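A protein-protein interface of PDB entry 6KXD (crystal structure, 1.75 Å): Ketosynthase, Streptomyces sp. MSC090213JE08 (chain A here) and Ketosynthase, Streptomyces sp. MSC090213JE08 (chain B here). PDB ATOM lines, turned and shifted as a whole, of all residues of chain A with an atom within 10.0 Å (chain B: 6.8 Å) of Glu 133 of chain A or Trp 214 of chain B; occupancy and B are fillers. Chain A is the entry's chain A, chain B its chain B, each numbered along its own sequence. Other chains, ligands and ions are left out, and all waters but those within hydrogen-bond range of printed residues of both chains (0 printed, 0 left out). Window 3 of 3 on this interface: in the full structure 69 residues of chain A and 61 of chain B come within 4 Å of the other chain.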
ATOM      1  N   LEU A 122      11.130   4.291 -16.385  1.00  0.00           N
ATOM      2  CA  LEU A 122      10.582   2.948 -16.340  1.00  0.00           C
ATOM      3  C   LEU A 122       9.735   2.639 -17.571  1.00  0.00           C
ATOM      4  O   LEU A 122       9.830   1.540 -18.136  1.00  0.00           O
ATOM      5  CB  LEU A 122       9.732   2.751 -15.080  1.00  0.00           C
ATOM      6  CG  LEU A 122      10.512   2.500 -13.799  1.00  0.00           C
ATOM      7  CD1 LEU A 122       9.625   2.743 -12.582  1.00  0.00           C
ATOM      8  CD2 LEU A 122      11.029   1.087 -13.805  1.00  0.00           C
ATOM      9  N   LEU A 123       8.843   3.564 -17.944  1.00  0.00           N
ATOM     10  CA  LEU A 123       7.999   3.294 -19.102  1.00  0.00           C
ATOM     11  C   LEU A 123       8.833   3.214 -20.390  1.00  0.00           C
ATOM     12  O   LEU A 123       8.464   2.461 -21.249  1.00  0.00           O
ATOM     13  CB  LEU A 123       6.947   4.393 -19.236  1.00  0.00           C
ATOM     14  CG  LEU A 123       5.931   4.387 -18.101  1.00  0.00           C
ATOM     15  CD1 LEU A 123       4.962   5.544 -18.265  1.00  0.00           C
ATOM     16  CD2 LEU A 123       5.210   3.047 -18.032  1.00  0.00           C
ATOM     17  N   GLN A 125      11.756   2.038 -20.592  1.00  0.00           N
ATOM     18  CA  GLN A 125      12.429   0.734 -20.616  1.00  0.00           C
ATOM     19  C   GLN A 125      11.456  -0.315 -21.156  1.00  0.00           C
ATOM     20  O   GLN A 125      11.831  -1.164 -21.985  1.00  0.00           O
ATOM     21  CB  GLN A 125      13.033   0.398 -19.255  1.00  0.00           C
ATOM     22  CG  GLN A 125      14.024   1.440 -18.758  1.00  0.00           C
ATOM     23  CD  GLN A 125      14.383   1.246 -17.305  1.00  0.00           C
ATOM     24  OE1 GLN A 125      13.633   0.607 -16.566  1.00  0.00           O
ATOM     25  NE2 GLN A 125      15.521   1.809 -16.894  1.00  0.00           N
ATOM     26  N   GLU A 126      10.188  -0.225 -20.738  1.00  0.00           N
ATOM     27  CA  GLU A 126       9.183  -1.145 -21.177  1.00  0.00           C
ATOM     28  C   GLU A 126       8.924  -0.913 -22.675  1.00  0.00           C
ATOM     29  O   GLU A 126       8.825  -1.865 -23.433  1.00  0.00           O
ATOM     30  CB  GLU A 126       7.874  -0.961 -20.409  1.00  0.00           C
ATOM     31  CG  GLU A 126       6.879  -2.077 -20.658  1.00  0.00           C
ATOM     32  CD  GLU A 126       5.609  -1.696 -21.383  1.00  0.00           C
ATOM     33  OE1 GLU A 126       5.690  -0.953 -22.387  1.00  0.00           O
ATOM     34  OE2 GLU A 126       4.533  -2.151 -20.933  1.00  0.00           O
ATOM     35  N   LEU A 127       8.860   0.357 -23.071  1.00  0.00           N
ATOM     36  CA  LEU A 127       8.526   0.721 -24.462  1.00  0.00           C
ATOM     37  C   LEU A 127       9.670   0.316 -25.407  1.00  0.00           C
ATOM     38  O   LEU A 127       9.408  -0.267 -26.443  1.00  0.00           O
ATOM     39  CB  LEU A 127       8.199   2.213 -24.549  1.00  0.00           C
ATOM     40  CG  LEU A 127       6.767   2.562 -24.145  1.00  0.00           C
ATOM     41  CD1 LEU A 127       6.604   4.048 -23.881  1.00  0.00           C
ATOM     42  CD2 LEU A 127       5.774   2.081 -25.188  1.00  0.00           C
ATOM     43  N   ALA A 128      10.925   0.600 -25.044  1.00  0.00           N
ATOM     44  CA  ALA A 128      12.099   0.148 -25.846  1.00  0.00           C
ATOM     45  C   ALA A 128      12.060  -1.374 -26.056  1.00  0.00           C
ATOM     46  O   ALA A 128      12.095  -1.840 -27.181  1.00  0.00           O
ATOM     47  CB  ALA A 128      13.392   0.555 -25.195  1.00  0.00           C
ATOM     48  N   ALA A 129      11.991  -2.141 -24.965  1.00  0.00           N
ATOM     49  CA  ALA A 129      12.002  -3.615 -25.015  1.00  0.00           C
ATOM     50  C   ALA A 129      10.683  -4.212 -25.548  1.00  0.00           C
ATOM     51  O   ALA A 129      10.641  -5.372 -25.938  1.00  0.00           O
ATOM     52  CB  ALA A 129      12.311  -4.138 -23.632  1.00  0.00           C
ATOM     53  N   GLY A 130       9.587  -3.446 -25.538  1.00  0.00           N
ATOM     54  CA  GLY A 130       8.249  -4.004 -25.743  1.00  0.00           C
ATOM     55  C   GLY A 130       7.896  -5.067 -24.708  1.00  0.00           C
ATOM     56  O   GLY A 130       7.166  -6.017 -25.005  1.00  0.00           O
ATOM     57  N   ASP A 131       8.404  -4.903 -23.478  1.00  0.00           N
ATOM     58  CA  ASP A 131       8.403  -5.978 -22.491  1.00  0.00           C
ATOM     59  C   ASP A 131       8.479  -5.381 -21.086  1.00  0.00           C
ATOM     60  O   ASP A 131       9.469  -4.720 -20.759  1.00  0.00           O
ATOM     61  CB  ASP A 131       9.583  -6.934 -22.713  1.00  0.00           C
ATOM     62  CG  ASP A 131       9.554  -8.216 -21.885  1.00  0.00           C
ATOM     63  OD1 ASP A 131       8.530  -8.486 -21.204  1.00  0.00           O
ATOM     64  OD2 ASP A 131      10.558  -8.956 -21.939  1.00  0.00           O
ATOM     65  N   PRO A 132       7.463  -5.617 -20.222  1.00  0.00           N
ATOM     66  CA  PRO A 132       7.471  -5.081 -18.859  1.00  0.00           C
ATOM     67  C   PRO A 132       8.709  -5.513 -18.057  1.00  0.00           C
ATOM     68  O   PRO A 132       9.193  -4.762 -17.240  1.00  0.00           O
ATOM     69  CB  PRO A 132       6.178  -5.642 -18.246  1.00  0.00           C
ATOM     70  CG  PRO A 132       5.277  -5.905 -19.435  1.00  0.00           C
ATOM     71  CD  PRO A 132       6.234  -6.383 -20.507  1.00  0.00           C
ATOM     72  N   GLU A 133       9.253  -6.692 -18.375  1.00  0.00           N
ATOM     73  CA  GLU A 133      10.322  -7.311 -17.614  1.00  0.00           C
ATOM     74  C   GLU A 133      11.657  -6.575 -17.817  1.00  0.00           C
ATOM     75  O   GLU A 133      12.613  -6.847 -17.117  1.00  0.00           O
ATOM     76  CB  GLU A 133      10.418  -8.788 -18.013  1.00  0.00           C
ATOM     77  CG  GLU A 133       9.094  -9.541 -17.925  1.00  0.00           C
ATOM     78  CD  GLU A 133       8.685  -9.961 -16.523  1.00  0.00           C
ATOM     79  OE1 GLU A 133       9.467  -9.700 -15.593  1.00  0.00           O
ATOM     80  OE2 GLU A 133       7.590 -10.564 -16.370  1.00  0.00           O
ATOM     81  N   ALA A 134      11.727  -5.636 -18.766  1.00  0.00           N
ATOM     82  CA  ALA A 134      12.925  -4.806 -19.001  1.00  0.00           C
ATOM     83  C   ALA A 134      13.042  -3.680 -17.959  1.00  0.00           C
ATOM     84  O   ALA A 134      14.033  -2.981 -17.875  1.00  0.00           O
ATOM     85  CB  ALA A 134      12.844  -4.220 -20.390  1.00  0.00           C
ATOM     86  N   MET A 135      11.986  -3.454 -17.176  1.00  0.00           N
ATOM     87  CA  MET A 135      12.013  -2.350 -16.246  1.00  0.00           C
ATOM     88  C   MET A 135      12.992  -2.631 -15.094  1.00  0.00           C
ATOM     89  O   MET A 135      13.057  -3.731 -14.577  1.00  0.00           O
ATOM     90  CB  MET A 135      10.600  -2.100 -15.732  1.00  0.00           C
ATOM     91  CG  MET A 135       9.808  -1.386 -16.774  1.00  0.00           C
ATOM     92  SD  MET A 135       8.187  -0.923 -16.189  1.00  0.00           S
ATOM     93  CE  MET A 135       7.417  -2.504 -15.865  1.00  0.00           C
ATOM     94  N   ASP A 136      13.730  -1.587 -14.720  1.00  0.00           N
ATOM     95  CA  ASP A 136      14.757  -1.665 -13.690  1.00  0.00           C
ATOM     96  C   ASP A 136      14.116  -1.721 -12.300  1.00  0.00           C
ATOM     97  O   ASP A 136      13.441  -0.777 -11.887  1.00  0.00           O
ATOM     98  CB  ASP A 136      15.716  -0.492 -13.849  1.00  0.00           C
ATOM     99  CG  ASP A 136      16.876  -0.468 -12.869  1.00  0.00           C
ATOM    100  OD1 ASP A 136      16.976  -1.386 -12.024  1.00  0.00           O
ATOM    101  OD2 ASP A 136      17.656   0.470 -12.947  1.00  0.00           O
ATOM    102  N   PRO A 137      14.368  -2.784 -11.500  1.00  0.00           N
ATOM    103  CA  PRO A 137      13.876  -2.848 -10.120  1.00  0.00           C
ATOM    104  C   PRO A 137      14.310  -1.630  -9.298  1.00  0.00           C
ATOM    105  O   PRO A 137      13.588  -1.231  -8.398  1.00  0.00           O
ATOM    106  CB  PRO A 137      14.493  -4.141  -9.585  1.00  0.00           C
ATOM    107  CG  PRO A 137      14.597  -4.988 -10.827  1.00  0.00           C
ATOM    108  CD  PRO A 137      15.111  -4.012 -11.861  1.00  0.00           C
ATOM    109  N   VAL A 138      15.489  -1.081  -9.586  1.00  0.00           N
ATOM    110  CA  VAL A 138      16.064  -0.039  -8.770  1.00  0.00           C
ATOM    111  C   VAL A 138      15.195   1.214  -8.903  1.00  0.00           C
ATOM    112  O   VAL A 138      14.920   1.903  -7.920  1.00  0.00           O
ATOM    113  CB  VAL A 138      17.538   0.222  -9.112  1.00  0.00           C
ATOM    114  CG1 VAL A 138      18.008   1.588  -8.684  1.00  0.00           C
ATOM    115  CG2 VAL A 138      18.410  -0.861  -8.503  1.00  0.00           C
ATOM    116  N   LEU A 139      14.761   1.478 -10.127  1.00  0.00           N
ATOM    117  CA  LEU A 139      13.830   2.540 -10.387  1.00  0.00           C
ATOM    118  C   LEU A 139      12.481   2.261  -9.742  1.00  0.00           C
ATOM    119  O   LEU A 139      11.929   3.180  -9.083  1.00  0.00           O
ATOM    120  CB  LEU A 139      13.632   2.705 -11.894  1.00  0.00           C
ATOM    121  CG  LEU A 139      14.790   3.342 -12.646  1.00  0.00           C
ATOM    122  CD1 LEU A 139      14.408   3.583 -14.099  1.00  0.00           C
ATOM    123  CD2 LEU A 139      15.188   4.637 -12.003  1.00  0.00           C
ATOM    124  N   ALA A 140      11.945   1.069  -9.941  1.00  0.00           N
ATOM    125  CA  ALA A 140      10.590   0.816  -9.496  1.00  0.00           C
ATOM    126  C   ALA A 140      10.544   0.905  -7.973  1.00  0.00           C
ATOM    127  O   ALA A 140       9.559   1.285  -7.445  1.00  0.00           O
ATOM    128  CB  ALA A 140      10.069  -0.505  -9.997  1.00  0.00           C
ATOM    129  N   ARG A 141      11.649   0.601  -7.286  1.00  0.00           N
ATOM    130  CA  ARG A 141      11.641   0.640  -5.800  1.00  0.00           C
ATOM    131  C   ARG A 141      11.605   2.064  -5.223  1.00  0.00           C
ATOM    132  O   ARG A 141      11.325   2.229  -4.057  1.00  0.00           O
ATOM    133  CB  ARG A 141      12.890  -0.068  -5.279  1.00  0.00           C
ATOM    134  CG  ARG A 141      12.698  -1.570  -5.329  1.00  0.00           C
ATOM    135  CD  ARG A 141      14.049  -2.252  -5.242  1.00  0.00           C
ATOM    136  NE  ARG A 141      13.884  -3.654  -5.569  1.00  0.00           N
ATOM    137  CZ  ARG A 141      14.888  -4.467  -5.837  1.00  0.00           C
ATOM    138  NH1 ARG A 141      16.112  -3.981  -5.926  1.00  0.00           N
ATOM    139  NH2 ARG A 141      14.652  -5.749  -6.010  1.00  0.00           N
ATOM    140  N   ILE A 143      10.012   4.991  -6.588  1.00  0.00           N
ATOM    141  CA  ILE A 143       9.070   5.933  -7.225  1.00  0.00           C
ATOM    142  C   ILE A 143       7.985   6.411  -6.257  1.00  0.00           C
ATOM    143  O   ILE A 143       7.320   7.362  -6.563  1.00  0.00           O
ATOM    144  CB  ILE A 143       8.416   5.338  -8.491  1.00  0.00           C
ATOM    145  CG1 ILE A 143       7.694   4.030  -8.192  1.00  0.00           C
ATOM    146  CG2 ILE A 143       9.467   5.182  -9.600  1.00  0.00           C
ATOM    147  CD1 ILE A 143       6.561   3.719  -9.113  1.00  0.00           C
ATOM    148  N   LEU B  56      -7.654  -5.444 -18.289  1.00  0.00           N
ATOM    149  CA  LEU B  56      -6.434  -4.880 -17.693  1.00  0.00           C
ATOM    150  C   LEU B  56      -5.186  -5.227 -18.518  1.00  0.00           C
ATOM    151  O   LEU B  56      -4.110  -4.718 -18.250  1.00  0.00           O
ATOM    152  CB  LEU B  56      -6.314  -5.410 -16.264  1.00  0.00           C
ATOM    153  CG  LEU B  56      -7.363  -4.851 -15.301  1.00  0.00           C
ATOM    154  CD1 LEU B  56      -7.555  -5.772 -14.110  1.00  0.00           C
ATOM    155  CD2 LEU B  56      -6.993  -3.442 -14.847  1.00  0.00           C
ATOM    156  N   GLY B  57      -5.323  -6.115 -19.510  1.00  0.00           N
ATOM    157  CA  GLY B  57      -4.204  -6.503 -20.351  1.00  0.00           C
ATOM    158  C   GLY B  57      -3.272  -7.432 -19.586  1.00  0.00           C
ATOM    159  O   GLY B  57      -3.609  -7.857 -18.484  1.00  0.00           O
ATOM    160  N   PRO B  58      -2.087  -7.779 -20.133  1.00  0.00           N
ATOM    161  CA  PRO B  58      -1.184  -8.708 -19.455  1.00  0.00           C
ATOM    162  C   PRO B  58      -0.825  -8.151 -18.065  1.00  0.00           C
ATOM    163  O   PRO B  58      -0.730  -6.942 -17.922  1.00  0.00           O
ATOM    164  CB  PRO B  58       0.041  -8.808 -20.385  1.00  0.00           C
ATOM    165  CG  PRO B  58      -0.061  -7.600 -21.318  1.00  0.00           C
ATOM    166  CD  PRO B  58      -1.540  -7.274 -21.401  1.00  0.00           C
ATOM    167  N   LEU B  59      -0.696  -9.046 -17.078  1.00  0.00           N
ATOM    168  CA  LEU B  59      -0.311  -8.724 -15.699  1.00  0.00           C
ATOM    169  C   LEU B  59       0.758  -9.706 -15.249  1.00  0.00           C
ATOM    170  O   LEU B  59       0.836 -10.812 -15.772  1.00  0.00           O
ATOM    171  CB  LEU B  59      -1.525  -8.834 -14.773  1.00  0.00           C
ATOM    172  CG  LEU B  59      -2.625  -7.799 -14.970  1.00  0.00           C
ATOM    173  CD1 LEU B  59      -3.873  -8.225 -14.227  1.00  0.00           C
ATOM    174  CD2 LEU B  59      -2.181  -6.414 -14.529  1.00  0.00           C
ATOM    175  N   PRO B  60       1.571  -9.359 -14.223  1.00  0.00           N
ATOM    176  CA  PRO B  60       2.611 -10.258 -13.734  1.00  0.00           C
ATOM    177  C   PRO B  60       2.023 -11.501 -13.059  1.00  0.00           C
ATOM    178  O   PRO B  60       2.722 -12.465 -12.857  1.00  0.00           O
ATOM    179  CB  PRO B  60       3.421  -9.451 -12.706  1.00  0.00           C
ATOM    180  CG  PRO B  60       2.738  -8.097 -12.592  1.00  0.00           C
ATOM    181  CD  PRO B  60       1.519  -8.092 -13.488  1.00  0.00           C
ATOM    182  N   SER B  61       0.758 -11.406 -12.652  1.00  0.00           N
ATOM    183  CA  SER B  61       0.016 -12.464 -12.063  1.00  0.00           C
ATOM    184  C   SER B  61      -1.441 -12.317 -12.484  1.00  0.00           C
ATOM    185  O   SER B  61      -1.950 -11.193 -12.635  1.00  0.00           O
ATOM    186  CB  SER B  61       0.137 -12.444 -10.568  1.00  0.00           C
ATOM    187  OG  SER B  61      -0.734 -13.411 -10.011  1.00  0.00           O
ATOM    188  N   SER B 209      -4.230  -1.385 -10.743  1.00  0.00           N
ATOM    189  CA  SER B 209      -3.946  -0.972 -12.113  1.00  0.00           C
ATOM    190  C   SER B 209      -2.841  -1.868 -12.636  1.00  0.00           C
ATOM    191  O   SER B 209      -2.017  -2.336 -11.858  1.00  0.00           O
ATOM    192  CB  SER B 209      -3.525   0.467 -12.270  1.00  0.00           C
ATOM    193  OG  SER B 209      -2.250   0.725 -11.694  1.00  0.00           O
ATOM    194  N   ALA B 210      -2.870  -2.126 -13.946  1.00  0.00           N
ATOM    195  CA  ALA B 210      -1.771  -2.880 -14.581  1.00  0.00           C
ATOM    196  C   ALA B 210      -0.434  -2.177 -14.293  1.00  0.00           C
ATOM    197  O   ALA B 210       0.597  -2.828 -14.025  1.00  0.00           O
ATOM    198  CB  ALA B 210      -2.025  -3.025 -16.076  1.00  0.00           C
ATOM    199  N   ALA B 211      -0.426  -0.847 -14.238  1.00  0.00           N
ATOM    200  CA  ALA B 211       0.820  -0.156 -13.985  1.00  0.00           C
ATOM    201  C   ALA B 211       1.376  -0.507 -12.598  1.00  0.00           C
ATOM    202  O   ALA B 211       2.561  -0.955 -12.426  1.00  0.00           O
ATOM    203  CB  ALA B 211       0.649   1.320 -14.188  1.00  0.00           C
ATOM    204  N   HIS B 212       0.527  -0.306 -11.596  1.00  0.00           N
ATOM    205  CA  HIS B 212       0.819  -0.685 -10.212  1.00  0.00           C
ATOM    206  C   HIS B 212       1.307  -2.132 -10.129  1.00  0.00           C
ATOM    207  O   HIS B 212       2.334  -2.396  -9.504  1.00  0.00           O
ATOM    208  CB  HIS B 212      -0.419  -0.475  -9.351  1.00  0.00           C
ATOM    209  CG  HIS B 212      -0.166  -0.739  -7.913  1.00  0.00           C
ATOM    210  ND1 HIS B 212      -0.875  -1.674  -7.217  1.00  0.00           N
ATOM    211  CD2 HIS B 212       0.763  -0.242  -7.083  1.00  0.00           C
ATOM    212  CE1 HIS B 212      -0.414  -1.713  -5.985  1.00  0.00           C
ATOM    213  NE2 HIS B 212       0.593  -0.854  -5.881  1.00  0.00           N
ATOM    214  N   ALA B 213       0.550  -3.058 -10.723  1.00  0.00           N
ATOM    215  CA  ALA B 213       0.885  -4.463 -10.644  1.00  0.00           C
ATOM    216  C   ALA B 213       2.281  -4.694 -11.237  1.00  0.00           C
ATOM    217  O   ALA B 213       3.102  -5.353 -10.626  1.00  0.00           O
ATOM    218  CB  ALA B 213      -0.143  -5.321 -11.328  1.00  0.00           C
ATOM    219  N   TRP B 214       2.542  -4.132 -12.416  1.00  0.00           N
ATOM    220  CA  TRP B 214       3.872  -4.302 -13.064  1.00  0.00           C
ATOM    221  C   TRP B 214       4.967  -3.613 -12.251  1.00  0.00           C
ATOM    222  O   TRP B 214       6.055  -4.165 -12.081  1.00  0.00           O
ATOM    223  CB  TRP B 214       3.794  -3.795 -14.512  1.00  0.00           C
ATOM    224  CG  TRP B 214       3.168  -4.812 -15.400  1.00  0.00           C
ATOM    225  CD1 TRP B 214       1.939  -4.780 -15.981  1.00  0.00           C
ATOM    226  CD2 TRP B 214       3.758  -6.072 -15.772  1.00  0.00           C
ATOM    227  NE1 TRP B 214       1.728  -5.930 -16.689  1.00  0.00           N
ATOM    228  CE2 TRP B 214       2.823  -6.737 -16.585  1.00  0.00           C
ATOM    229  CE3 TRP B 214       4.981  -6.695 -15.478  1.00  0.00           C
ATOM    230  CZ2 TRP B 214       3.076  -7.999 -17.127  1.00  0.00           C
ATOM    231  CZ3 TRP B 214       5.233  -7.940 -16.021  1.00  0.00           C
ATOM    232  CH2 TRP B 214       4.283  -8.584 -16.808  1.00  0.00           C
ATOM    233  N   PHE B 215       4.691  -2.428 -11.698  1.00  0.00           N
ATOM    234  CA  PHE B 215       5.732  -1.747 -10.961  1.00  0.00           C
ATOM    235  C   PHE B 215       6.071  -2.516  -9.691  1.00  0.00           C
ATOM    236  O   PHE B 215       7.246  -2.592  -9.308  1.00  0.00           O
ATOM    237  CB  PHE B 215       5.347  -0.316 -10.617  1.00  0.00           C
ATOM    238  CG  PHE B 215       5.428   0.648 -11.769  1.00  0.00           C
ATOM    239  CD1 PHE B 215       6.069   0.314 -12.948  1.00  0.00           C
ATOM    240  CD2 PHE B 215       4.858   1.907 -11.667  1.00  0.00           C
ATOM    241  CE1 PHE B 215       6.138   1.215 -14.001  1.00  0.00           C
ATOM    242  CE2 PHE B 215       4.935   2.804 -12.723  1.00  0.00           C
ATOM    243  CZ  PHE B 215       5.600   2.462 -13.875  1.00  0.00           C
ATOM    244  N   GLU B 216       5.039  -3.035  -9.033  1.00  0.00           N
ATOM    245  CA  GLU B 216       5.223  -3.828  -7.821  1.00  0.00           C
ATOM    246  C   GLU B 216       6.088  -5.043  -8.130  1.00  0.00           C
ATOM    247  O   GLU B 216       6.955  -5.401  -7.349  1.00  0.00           O
ATOM    248  CB  GLU B 216       3.880  -4.318  -7.282  1.00  0.00           C
ATOM    249  CG  GLU B 216       3.184  -3.260  -6.449  1.00  0.00           C
ATOM    250  CD  GLU B 216       3.995  -2.793  -5.254  1.00  0.00           C
ATOM    251  OE1 GLU B 216       4.264  -3.627  -4.355  1.00  0.00           O
ATOM    252  OE2 GLU B 216       4.394  -1.617  -5.256  1.00  0.00           O
ATOM    253  N   HIS B 217       5.729  -5.737  -9.208  1.00  0.00           N
ATOM    254  CA  HIS B 217       6.461  -6.937  -9.648  1.00  0.00           C
ATOM    255  C   HIS B 217       7.934  -6.581  -9.892  1.00  0.00           C
ATOM    256  O   HIS B 217       8.826  -7.287  -9.432  1.00  0.00           O
ATOM    257  CB  HIS B 217       5.790  -7.553 -10.878  1.00  0.00           C
ATOM    258  CG  HIS B 217       6.668  -8.494 -11.642  1.00  0.00           C
ATOM    259  ND1 HIS B 217       6.838  -9.813 -11.263  1.00  0.00           N
ATOM    260  CD2 HIS B 217       7.402  -8.319 -12.765  1.00  0.00           C
ATOM    261  CE1 HIS B 217       7.656 -10.407 -12.110  1.00  0.00           C
ATOM    262  NE2 HIS B 217       8.033  -9.504 -13.030  1.00  0.00           N
ATOM    263  N   THR B 218       8.173  -5.460 -10.575  1.00  0.00           N
ATOM    264  CA  THR B 218       9.499  -4.992 -10.862  1.00  0.00           C
ATOM    265  C   THR B 218      10.260  -4.746  -9.554  1.00  0.00           C
ATOM    266  O   THR B 218      11.409  -5.124  -9.453  1.00  0.00           O
ATOM    267  CB  THR B 218       9.490  -3.717 -11.708  1.00  0.00           C
ATOM    268  OG1 THR B 218       8.641  -3.892 -12.838  1.00  0.00           O
ATOM    269  CG2 THR B 218      10.859  -3.308 -12.191  1.00  0.00           C
ATOM    270  N   ALA B 219       9.600  -4.090  -8.579  1.00  0.00           N
ATOM    271  CA  ALA B 219      10.209  -3.679  -7.317  1.00  0.00           C
ATOM    272  C   ALA B 219      10.470  -4.881  -6.394  1.00  0.00           C
ATOM    273  O   ALA B 219      11.290  -4.769  -5.476  1.00  0.00           O
ATOM    274  CB  ALA B 219       9.348  -2.647  -6.613  1.00  0.00           C
ATOM    275  N   LEU B 229      -2.168  -8.711  -5.247  1.00  0.00           N
ATOM    276  CA  LEU B 229      -2.431  -7.281  -5.010  1.00  0.00           C
ATOM    277  C   LEU B 229      -3.936  -7.089  -4.844  1.00  0.00           C
ATOM    278  O   LEU B 229      -4.730  -7.668  -5.565  1.00  0.00           O
ATOM    279  CB  LEU B 229      -1.911  -6.461  -6.188  1.00  0.00           C
ATOM    280  CG  LEU B 229      -0.389  -6.429  -6.320  1.00  0.00           C
ATOM    281  CD1 LEU B 229       0.034  -5.742  -7.605  1.00  0.00           C
ATOM    282  CD2 LEU B 229       0.234  -5.738  -5.106  1.00  0.00           C
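The side-chain carboxylate of Glu 133 of chain A is in hydrogen-bond range of a ring nitrogen (NE2) of His 217 of chain B (2.9 Å). NE of Arg 141 of chain A lies within hydrogen-bond range of O of Ala 219 of chain B (2.8 Å).
The backbone NH of Val 138 of chain A lies within hydrogen-bond range of the side-chain carboxylate of Asp 136 of chain A (2.9 Å). OD1 of Asp 131 of chain A lies close to N of Glu 133 of chain A, at 3.4 Å. The side-chain amide oxygen (OE1) of Gln 125 of chain A sits at hydrogen-bond distance from the backbone NH (N) of Asp 136 of chain A, at 2.9 Å. O of Trp 214 of chain B lies within hydrogen-bond range of OG1 of Thr 218 of chain B, 2.7 Å away. The indole nitrogen (NE1) of Trp 214 of chain B lies within hydrogen-bond range of the backbone carbonyl oxygen (O) of Pro 58 of chain B (2.9 Å).
Among the printed residues, pairs that only touch across the chains: Pro 132 of chain A with Trp 214 of chain B (3.2 Å), Glu 133 of chain A with Trp 214 of chain B (3.5 Å), Met 135 of chain A with Phe 215 of chain B (3.7 Å), Met 135 of chain A with Thr 218 of chain B (3.3 Å), Asp 136 of chain A with Thr 218 of chain B (3.6 Å), Pro 137 of chain A with Thr 218 of chain B (3.2 Å), Ala 140 of chain A with Phe 215 of chain B (3.6 Å), Ala 140 of chain A with Thr 218 of chain B (3.6 Å), Ala 140 of chain A with Ala 219 of chain B (3.9 Å) and Ile 143 of chain A with Phe 215 of chain B (3.6 Å).
Glu 133 of chain A touches just these residues of chain B: Trp 214 and His 217. Trp 214 of chain B touches just these residues of chain A: Pro 132 and Glu 133. No residue of chain A comes within 4 Å of Pro 60 of chain B. Ala 210 of chain B touches none of the printed residues of chain A. His 217 of chain B touches just one residue of chain A: Glu 133 (2.9 Å). Of the printed residues of chain B, Arg 141 of chain A touches Ala 219 (2.8 Å). Of the printed residues of chain A, Phe 215 of chain B touches Met 135, Ala 140 and Ile 143. Printed residues of chain B within 4 Å of Met 135 of chain A: Phe 215 and Thr 218. Of the printed residues of chain A, Thr 218 of chain B touches Met 135, Asp 136, Pro 137 and Ala 140. Printed residues of chain B within 4 Å of Pro 137 of chain A: Thr 218. Leu 123 of chain A touches none of the printed residues of chain B. Gly 57 of chain B touches none of the printed residues of chain A.
Of the 18 printed residues of chain B, 5 touch a printed residue of chain A. Hydrophobic or aromatic side chains of chain B within 4 Å of the printed part of chain A: Trp 214, Phe 215, His 217 and Ala 219. Among the printed residues, 12 pairs touch across the chains.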
